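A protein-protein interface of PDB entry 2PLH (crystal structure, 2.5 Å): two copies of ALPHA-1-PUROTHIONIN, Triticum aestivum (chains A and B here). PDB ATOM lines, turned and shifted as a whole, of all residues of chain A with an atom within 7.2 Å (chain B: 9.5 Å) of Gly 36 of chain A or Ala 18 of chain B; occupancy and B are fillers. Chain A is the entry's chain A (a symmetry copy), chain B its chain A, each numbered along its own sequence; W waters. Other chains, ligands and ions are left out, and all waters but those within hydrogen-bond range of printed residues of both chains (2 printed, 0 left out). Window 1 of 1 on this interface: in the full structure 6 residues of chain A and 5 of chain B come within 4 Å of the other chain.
Ser 35 of chain A touches Ala 21 of chain B. Gly 36 of chain A touches Arg 17 of chain B (CA to O, 2.9 Å). O of Ala 18 of chain B touches CA of Gly 36 of chain A (3.4 Å). Gly 20 of chain B touches Gly 36 of chain A. NH2 of Arg 19 of chain B touches C of Cys 39 of chain A, 3.0 Å away.
Of the 9 printed residues of chain A, 6 touch a printed residue of chain B. Hydrophobic or aromatic side chains of chain A within 4 Å of the printed part of chain B: Leu 37 and Pro 40. Of the 15 printed residues of chain B, 5 touch a printed residue of chain A. Hydrophobic or aromatic side chains of chain B that line the printed part of chain A: Ala 18 and Ala 21.
The backbone carbonyl oxygen (O) of Gly 20 of chain B sits at hydrogen-bond distance from the guanidinium group (NH1) of Arg 17 of chain B. N of Arg 17 of chain B sits at hydrogen-bond distance from SG of Cys 25 of chain B, at 3.4 Å. The side-chain amino group (NZ) of Lys 1 of chain A lies within hydrogen-bond range of the side-chain sulfur (SG) of Cys 39 of chain A. The side-chain sulfur of Cys 25 of chain B forms a disulfide with the side-chain sulfur of Cys 16 of chain B (2.0 Å).
Water W1 lies within hydrogen-bond range of the guanidinium group of Arg 19 of chain B, the backbone carbonyl oxygen of Ser 38 of chain A and the side-chain hydroxyl of Ser 34 of chain A. Water W2 lies within hydrogen-bond range of the guanidinium group (NH1) of Arg 17 of chain B (3.2 Å), the backbone carbonyl oxygen (O) of Ser 35 of chain A (3.4 Å) and the backbone NH (N) of Gln 22 of chain B (3.4 Å).
No position is printed for both chains.
Of chain B, only Arg 17 (2.9 Å), Ala 18 (3.4 Å) and Gly 20 (3.3 Å) come within 4 Å of Gly 36 of chain A. Ala 18 of chain B touches three residues of chain A. Of chain B, only Arg 17 and Ala 21 come within 4 Å of Ser 35 of chain A. Of chain B, only Arg 17 (2.7 Å) and Ala 18 (3.0 Å) come within 4 Å of Leu 37 of chain A. Ser 38 of chain A touches just these residues of chain B: Ala 18 and Arg 19. Of the printed residues of chain B, Pro 40 of chain A touches Arg 19. Of the printed residues of chain A, Arg 17 of chain B touches Ser 35 (3.2 Å), Gly 36 (2.9 Å) and Leu 37 (2.7 Å). Printed residues of chain B within 4 Å of Cys 39 of chain A: Arg 19. Of the printed residues of chain A, Gly 20 of chain B touches Gly 36 (3.3 Å). Of the printed residues of chain A, Arg 19 of chain B touches Ser 38 (2.8 Å), Cys 39 (3.0 Å) and Pro 40 (2.7 Å). The nearest residue of chain B that does not touch Gly 36 of chain A is Arg 19 of chain B (4.1 Å).
The backbone NH (N) of Leu 37 of chain A is in hydrogen-bond range of the backbone carbonyl oxygen (O) of Arg 17 of chain B (2.7 Å). The backbone carbonyl oxygen (O) of Ala 18 of chain B sits at hydrogen-bond distance from the backbone NH (N) of Leu 37 of chain A. N of Ser 38 of chain A is in hydrogen-bond range of O of Ala 18 of chain B (2.6 Å). NH2 of Arg 19 of chain B sits close to N of Pro 40 of chain A. The backbone carbonyl oxygen (O) of Ser 35 of chain A is in hydrogen-bond range of the guanidinium group (NH1) of Arg 17 of chain B (3.2 Å). NH2 of Arg 19 of chain B lies within hydrogen-bond range of O of Ser 38 of chain A, 2.8 Å away.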
ATOM      1  N   LYS A   1       1.169 -23.157  -7.796  1.00  0.00           N
ATOM      2  CA  LYS A   1       0.892 -24.278  -8.706  1.00  0.00           C
ATOM      3  C   LYS A   1       2.204 -24.847  -9.216  1.00  0.00           C
ATOM      4  O   LYS A   1       3.114 -24.098  -9.627  1.00  0.00           O
ATOM      5  CB  LYS A   1       0.008 -23.827  -9.859  1.00  0.00           C
ATOM      6  CG  LYS A   1      -1.173 -24.768 -10.105  1.00  0.00           C
ATOM      7  CD  LYS A   1      -1.390 -24.960 -11.595  1.00  0.00           C
ATOM      8  CE  LYS A   1      -2.141 -26.253 -11.881  1.00  0.00           C
ATOM      9  NZ  LYS A   1      -1.462 -26.987 -12.989  1.00  0.00           N
ATOM     10  N   ILE A  33       7.105 -23.525  -9.427  1.00  0.00           N
ATOM     11  CA  ILE A  33       5.888 -23.150  -8.665  1.00  0.00           C
ATOM     12  C   ILE A  33       5.504 -21.724  -9.021  1.00  0.00           C
ATOM     13  O   ILE A  33       6.193 -20.769  -8.634  1.00  0.00           O
ATOM     14  CB  ILE A  33       6.177 -23.446  -7.161  1.00  0.00           C
ATOM     15  CG1 ILE A  33       6.102 -24.982  -6.946  1.00  0.00           C
ATOM     16  CG2 ILE A  33       5.258 -22.649  -6.202  1.00  0.00           C
ATOM     17  CD1 ILE A  33       7.073 -25.471  -5.844  1.00  0.00           C
ATOM     18  N   SER A  34       4.424 -21.594  -9.772  1.00  0.00           N
ATOM     19  CA  SER A  34       3.982 -20.256 -10.219  1.00  0.00           C
ATOM     20  C   SER A  34       2.971 -19.626  -9.286  1.00  0.00           C
ATOM     21  O   SER A  34       2.416 -20.278  -8.385  1.00  0.00           O
ATOM     22  CB  SER A  34       3.576 -20.265 -11.677  1.00  0.00           C
ATOM     23  OG  SER A  34       2.674 -21.265 -12.064  1.00  0.00           O
ATOM     24  N   SER A  35       2.759 -18.331  -9.533  1.00  0.00           N
ATOM     25  CA  SER A  35       1.833 -17.487  -8.776  1.00  0.00           C
ATOM     26  C   SER A  35       0.424 -17.540  -9.390  1.00  0.00           C
ATOM     27  O   SER A  35      -0.566 -17.620  -8.636  1.00  0.00           O
ATOM     28  CB  SER A  35       2.296 -16.040  -8.710  1.00  0.00           C
ATOM     29  OG  SER A  35       3.598 -15.887  -8.198  1.00  0.00           O
ATOM     30  N   GLY A  36       0.410 -17.463 -10.716  1.00  0.00           N
ATOM     31  CA  GLY A  36      -0.828 -17.498 -11.493  1.00  0.00           C
ATOM     32  C   GLY A  36      -1.543 -18.822 -11.223  1.00  0.00           C
ATOM     33  O   GLY A  36      -1.197 -19.566 -10.285  1.00  0.00           O
ATOM     34  N   LEU A  37      -2.541 -19.097 -12.030  1.00  0.00           N
ATOM     35  CA  LEU A  37      -3.360 -20.310 -11.959  1.00  0.00           C
ATOM     36  C   LEU A  37      -3.040 -21.239 -13.141  1.00  0.00           C
ATOM     37  O   LEU A  37      -3.389 -22.428 -13.113  1.00  0.00           O
ATOM     38  CB  LEU A  37      -4.822 -19.916 -11.882  1.00  0.00           C
ATOM     39  CG  LEU A  37      -5.348 -18.865 -10.946  1.00  0.00           C
ATOM     40  CD1 LEU A  37      -6.705 -18.304 -11.441  1.00  0.00           C
ATOM     41  CD2 LEU A  37      -5.559 -19.496  -9.568  1.00  0.00           C
ATOM     42  N   SER A  38      -2.418 -20.703 -14.160  1.00  0.00           N
ATOM     43  CA  SER A  38      -1.976 -21.343 -15.384  1.00  0.00           C
ATOM     44  C   SER A  38      -0.472 -21.641 -15.313  1.00  0.00           C
ATOM     45  O   SER A  38       0.341 -20.879 -14.789  1.00  0.00           O
ATOM     46  CB  SER A  38      -2.282 -20.483 -16.599  1.00  0.00           C
ATOM     47  OG  SER A  38      -1.367 -20.658 -17.675  1.00  0.00           O
ATOM     48  N   CYS A  39      -0.120 -22.763 -15.870  1.00  0.00           N
ATOM     49  CA  CYS A  39       1.225 -23.312 -15.964  1.00  0.00           C
ATOM     50  C   CYS A  39       1.881 -22.903 -17.282  1.00  0.00           C
ATOM     51  O   CYS A  39       1.282 -23.098 -18.356  1.00  0.00           O
ATOM     52  CB  CYS A  39       1.125 -24.849 -15.878  1.00  0.00           C
ATOM     53  SG  CYS A  39       1.269 -25.489 -14.191  1.00  0.00           S
ATOM     54  N   PRO A  40       3.094 -22.382 -17.177  1.00  0.00           N
ATOM     55  CA  PRO A  40       3.886 -21.951 -18.340  1.00  0.00           C
ATOM     56  C   PRO A  40       3.902 -22.994 -19.441  1.00  0.00           C
ATOM     57  O   PRO A  40       3.547 -24.172 -19.213  1.00  0.00           O
ATOM     58  CB  PRO A  40       5.269 -21.708 -17.750  1.00  0.00           C
ATOM     59  CG  PRO A  40       4.938 -21.214 -16.341  1.00  0.00           C
ATOM     60  CD  PRO A  40       3.816 -22.162 -15.905  1.00  0.00           C
ATOM     61  N   ASN B  11     -12.012  -8.608 -16.521  1.00  0.00           N
ATOM     62  CA  ASN B  11     -11.552  -9.501 -17.607  1.00  0.00           C
ATOM     63  C   ASN B  11     -10.032  -9.530 -17.524  1.00  0.00           C
ATOM     64  O   ASN B  11      -9.407 -10.573 -17.269  1.00  0.00           O
ATOM     65  CB  ASN B  11     -12.157  -9.033 -18.924  1.00  0.00           C
ATOM     66  CG  ASN B  11     -13.589  -9.483 -19.164  1.00  0.00           C
ATOM     67  OD1 ASN B  11     -14.372  -9.726 -18.235  1.00  0.00           O
ATOM     68  ND2 ASN B  11     -13.990  -9.605 -20.432  1.00  0.00           N
ATOM     69  N   CYS B  12      -9.505  -8.334 -17.730  1.00  0.00           N
ATOM     70  CA  CYS B  12      -8.056  -8.104 -17.682  1.00  0.00           C
ATOM     71  C   CYS B  12      -7.469  -8.796 -16.454  1.00  0.00           C
ATOM     72  O   CYS B  12      -6.338  -9.336 -16.552  1.00  0.00           O
ATOM     73  CB  CYS B  12      -7.756  -6.604 -17.671  1.00  0.00           C
ATOM     74  SG  CYS B  12      -6.093  -6.082 -17.243  1.00  0.00           S
ATOM     75  N   TYR B  13      -8.223  -8.742 -15.360  1.00  0.00           N
ATOM     76  CA  TYR B  13      -7.733  -9.337 -14.122  1.00  0.00           C
ATOM     77  C   TYR B  13      -7.832 -10.849 -14.053  1.00  0.00           C
ATOM     78  O   TYR B  13      -6.922 -11.527 -13.541  1.00  0.00           O
ATOM     79  CB  TYR B  13      -8.388  -8.691 -12.880  1.00  0.00           C
ATOM     80  CG  TYR B  13      -7.848  -9.303 -11.600  1.00  0.00           C
ATOM     81  CD1 TYR B  13      -8.340 -10.493 -11.071  1.00  0.00           C
ATOM     82  CD2 TYR B  13      -6.807  -8.662 -10.922  1.00  0.00           C
ATOM     83  CE1 TYR B  13      -7.818 -11.033  -9.892  1.00  0.00           C
ATOM     84  CE2 TYR B  13      -6.274  -9.190  -9.748  1.00  0.00           C
ATOM     85  CZ  TYR B  13      -6.785 -10.376  -9.230  1.00  0.00           C
ATOM     86  OH  TYR B  13      -6.231 -10.844  -8.070  1.00  0.00           O
ATOM     87  N   ASN B  14      -8.926 -11.394 -14.521  1.00  0.00           N
ATOM     88  CA  ASN B  14      -9.161 -12.848 -14.488  1.00  0.00           C
ATOM     89  C   ASN B  14      -8.250 -13.610 -15.434  1.00  0.00           C
ATOM     90  O   ASN B  14      -7.973 -14.788 -15.200  1.00  0.00           O
ATOM     91  CB  ASN B  14     -10.637 -13.103 -14.774  1.00  0.00           C
ATOM     92  CG  ASN B  14     -11.570 -13.014 -13.604  1.00  0.00           C
ATOM     93  OD1 ASN B  14     -11.212 -12.802 -12.444  1.00  0.00           O
ATOM     94  ND2 ASN B  14     -12.864 -13.201 -13.924  1.00  0.00           N
ATOM     95  N   LEU B  15      -7.854 -12.921 -16.463  1.00  0.00           N
ATOM     96  CA  LEU B  15      -7.007 -13.357 -17.586  1.00  0.00           C
ATOM     97  C   LEU B  15      -5.541 -13.157 -17.318  1.00  0.00           C
ATOM     98  O   LEU B  15      -4.710 -13.835 -17.947  1.00  0.00           O
ATOM     99  CB  LEU B  15      -7.636 -12.652 -18.773  1.00  0.00           C
ATOM    100  CG  LEU B  15      -7.104 -12.631 -20.166  1.00  0.00           C
ATOM    101  CD1 LEU B  15      -7.579 -13.816 -20.999  1.00  0.00           C
ATOM    102  CD2 LEU B  15      -7.527 -11.302 -20.831  1.00  0.00           C
ATOM    103  N   CYS B  16      -5.198 -12.256 -16.403  1.00  0.00           N
ATOM    104  CA  CYS B  16      -3.800 -11.977 -16.020  1.00  0.00           C
ATOM    105  C   CYS B  16      -3.341 -13.037 -15.004  1.00  0.00           C
ATOM    106  O   CYS B  16      -2.188 -13.486 -15.058  1.00  0.00           O
ATOM    107  CB  CYS B  16      -3.543 -10.581 -15.502  1.00  0.00           C
ATOM    108  SG  CYS B  16      -1.986 -10.396 -14.528  1.00  0.00           S
ATOM    109  N   ARG B  17      -4.246 -13.404 -14.123  1.00  0.00           N
ATOM    110  CA  ARG B  17      -4.103 -14.374 -13.063  1.00  0.00           C
ATOM    111  C   ARG B  17      -3.721 -15.781 -13.523  1.00  0.00           C
ATOM    112  O   ARG B  17      -3.379 -16.660 -12.689  1.00  0.00           O
ATOM    113  CB  ARG B  17      -5.371 -14.468 -12.203  1.00  0.00           C
ATOM    114  CG  ARG B  17      -5.612 -13.404 -11.182  1.00  0.00           C
ATOM    115  CD  ARG B  17      -4.712 -13.379 -10.019  1.00  0.00           C
ATOM    116  NE  ARG B  17      -4.671 -14.610  -9.271  1.00  0.00           N
ATOM    117  CZ  ARG B  17      -3.619 -15.308  -8.871  1.00  0.00           C
ATOM    118  NH1 ARG B  17      -2.361 -14.990  -9.141  1.00  0.00           N
ATOM    119  NH2 ARG B  17      -3.881 -16.395  -8.136  1.00  0.00           N
ATOM    120  N   ALA B  18      -3.801 -15.997 -14.821  1.00  0.00           N
ATOM    121  CA  ALA B  18      -3.436 -17.307 -15.401  1.00  0.00           C
ATOM    122  C   ALA B  18      -1.913 -17.411 -15.252  1.00  0.00           C
ATOM    123  O   ALA B  18      -1.341 -18.367 -14.727  1.00  0.00           O
ATOM    124  CB  ALA B  18      -3.898 -17.395 -16.835  1.00  0.00           C
ATOM    125  N   ARG B  19      -1.253 -16.359 -15.694  1.00  0.00           N
ATOM    126  CA  ARG B  19       0.176 -16.155 -15.727  1.00  0.00           C
ATOM    127  C   ARG B  19       0.796 -15.352 -14.601  1.00  0.00           C
ATOM    128  O   ARG B  19       1.936 -15.684 -14.205  1.00  0.00           O
ATOM    129  CB  ARG B  19       0.598 -15.403 -17.019  1.00  0.00           C
ATOM    130  CG  ARG B  19       0.014 -15.898 -18.319  1.00  0.00           C
ATOM    131  CD  ARG B  19       0.403 -17.212 -18.833  1.00  0.00           C
ATOM    132  NE  ARG B  19       0.772 -18.209 -17.853  1.00  0.00           N
ATOM    133  CZ  ARG B  19       1.704 -19.138 -17.964  1.00  0.00           C
ATOM    134  NH1 ARG B  19       2.466 -19.341 -19.042  1.00  0.00           N
ATOM    135  NH2 ARG B  19       1.911 -19.949 -16.908  1.00  0.00           N
ATOM    136  N   GLY B  20       0.120 -14.328 -14.128  1.00  0.00           N
ATOM    137  CA  GLY B  20       0.636 -13.454 -13.085  1.00  0.00           C
ATOM    138  C   GLY B  20       0.040 -13.602 -11.716  1.00  0.00           C
ATOM    139  O   GLY B  20      -1.035 -14.176 -11.504  1.00  0.00           O
ATOM    140  N   ALA B  21       0.789 -13.050 -10.776  1.00  0.00           N
ATOM    141  CA  ALA B  21       0.487 -13.023  -9.346  1.00  0.00           C
ATOM    142  C   ALA B  21      -0.670 -12.059  -9.114  1.00  0.00           C
ATOM    143  O   ALA B  21      -1.132 -11.362 -10.027  1.00  0.00           O
ATOM    144  CB  ALA B  21       1.711 -12.606  -8.528  1.00  0.00           C
ATOM    145  N   GLN B  22      -1.133 -12.021  -7.896  1.00  0.00           N
ATOM    146  CA  GLN B  22      -2.217 -11.200  -7.408  1.00  0.00           C
ATOM    147  C   GLN B  22      -1.930  -9.707  -7.513  1.00  0.00           C
ATOM    148  O   GLN B  22      -2.718  -8.988  -8.151  1.00  0.00           O
ATOM    149  CB  GLN B  22      -2.516 -11.584  -5.948  1.00  0.00           C
ATOM    150  CG  GLN B  22      -3.461 -12.716  -5.799  1.00  0.00           C
ATOM    151  CD  GLN B  22      -4.194 -12.962  -4.540  1.00  0.00           C
ATOM    152  OE1 GLN B  22      -4.965 -13.952  -4.442  1.00  0.00           O
ATOM    153  NE2 GLN B  22      -4.056 -12.129  -3.508  1.00  0.00           N
ATOM    154  N   LYS B  23      -0.837  -9.287  -6.897  1.00  0.00           N
ATOM    155  CA  LYS B  23      -0.419  -7.892  -6.868  1.00  0.00           C
ATOM    156  C   LYS B  23       0.014  -7.356  -8.216  1.00  0.00           C
ATOM    157  O   LYS B  23      -0.246  -6.169  -8.463  1.00  0.00           O
ATOM    158  CB  LYS B  23       0.650  -7.597  -5.837  1.00  0.00           C
ATOM    159  CG  LYS B  23       0.180  -7.543  -4.384  1.00  0.00           C
ATOM    160  CD  LYS B  23       1.389  -7.277  -3.486  1.00  0.00           C
ATOM    161  CE  LYS B  23       1.094  -7.555  -2.019  1.00  0.00           C
ATOM    162  NZ  LYS B  23       2.412  -7.777  -1.342  1.00  0.00           N
ATOM    163  N   LEU B  24       0.646  -8.169  -9.040  1.00  0.00           N
ATOM    164  CA  LEU B  24       1.064  -7.655 -10.355  1.00  0.00           C
ATOM    165  C   LEU B  24      -0.187  -7.288 -11.160  1.00  0.00           C
ATOM    166  O   LEU B  24      -0.239  -6.205 -11.733  1.00  0.00           O
ATOM    167  CB  LEU B  24       1.943  -8.639 -11.118  1.00  0.00           C
ATOM    168  CG  LEU B  24       1.660  -8.634 -12.619  1.00  0.00           C
ATOM    169  CD1 LEU B  24       2.455  -7.548 -13.344  1.00  0.00           C
ATOM    170  CD2 LEU B  24       1.992  -9.984 -13.211  1.00  0.00           C
ATOM    171  N   CYS B  25      -1.123  -8.220 -11.165  1.00  0.00           N
ATOM    172  CA  CYS B  25      -2.400  -8.126 -11.868  1.00  0.00           C
ATOM    173  C   CYS B  25      -3.291  -7.027 -11.291  1.00  0.00           C
ATOM    174  O   CYS B  25      -3.984  -6.352 -12.059  1.00  0.00           O
ATOM    175  CB  CYS B  25      -3.201  -9.410 -11.865  1.00  0.00           C
ATOM    176  SG  CYS B  25      -2.579 -10.842 -12.670  1.00  0.00           S
HETATM  177  O   HOH W   1       2.540 -19.049 -14.411  1.00  0.00           O
HETATM  178  O   HOH W   2      -0.705 -15.058  -6.397  1.00  0.00           O
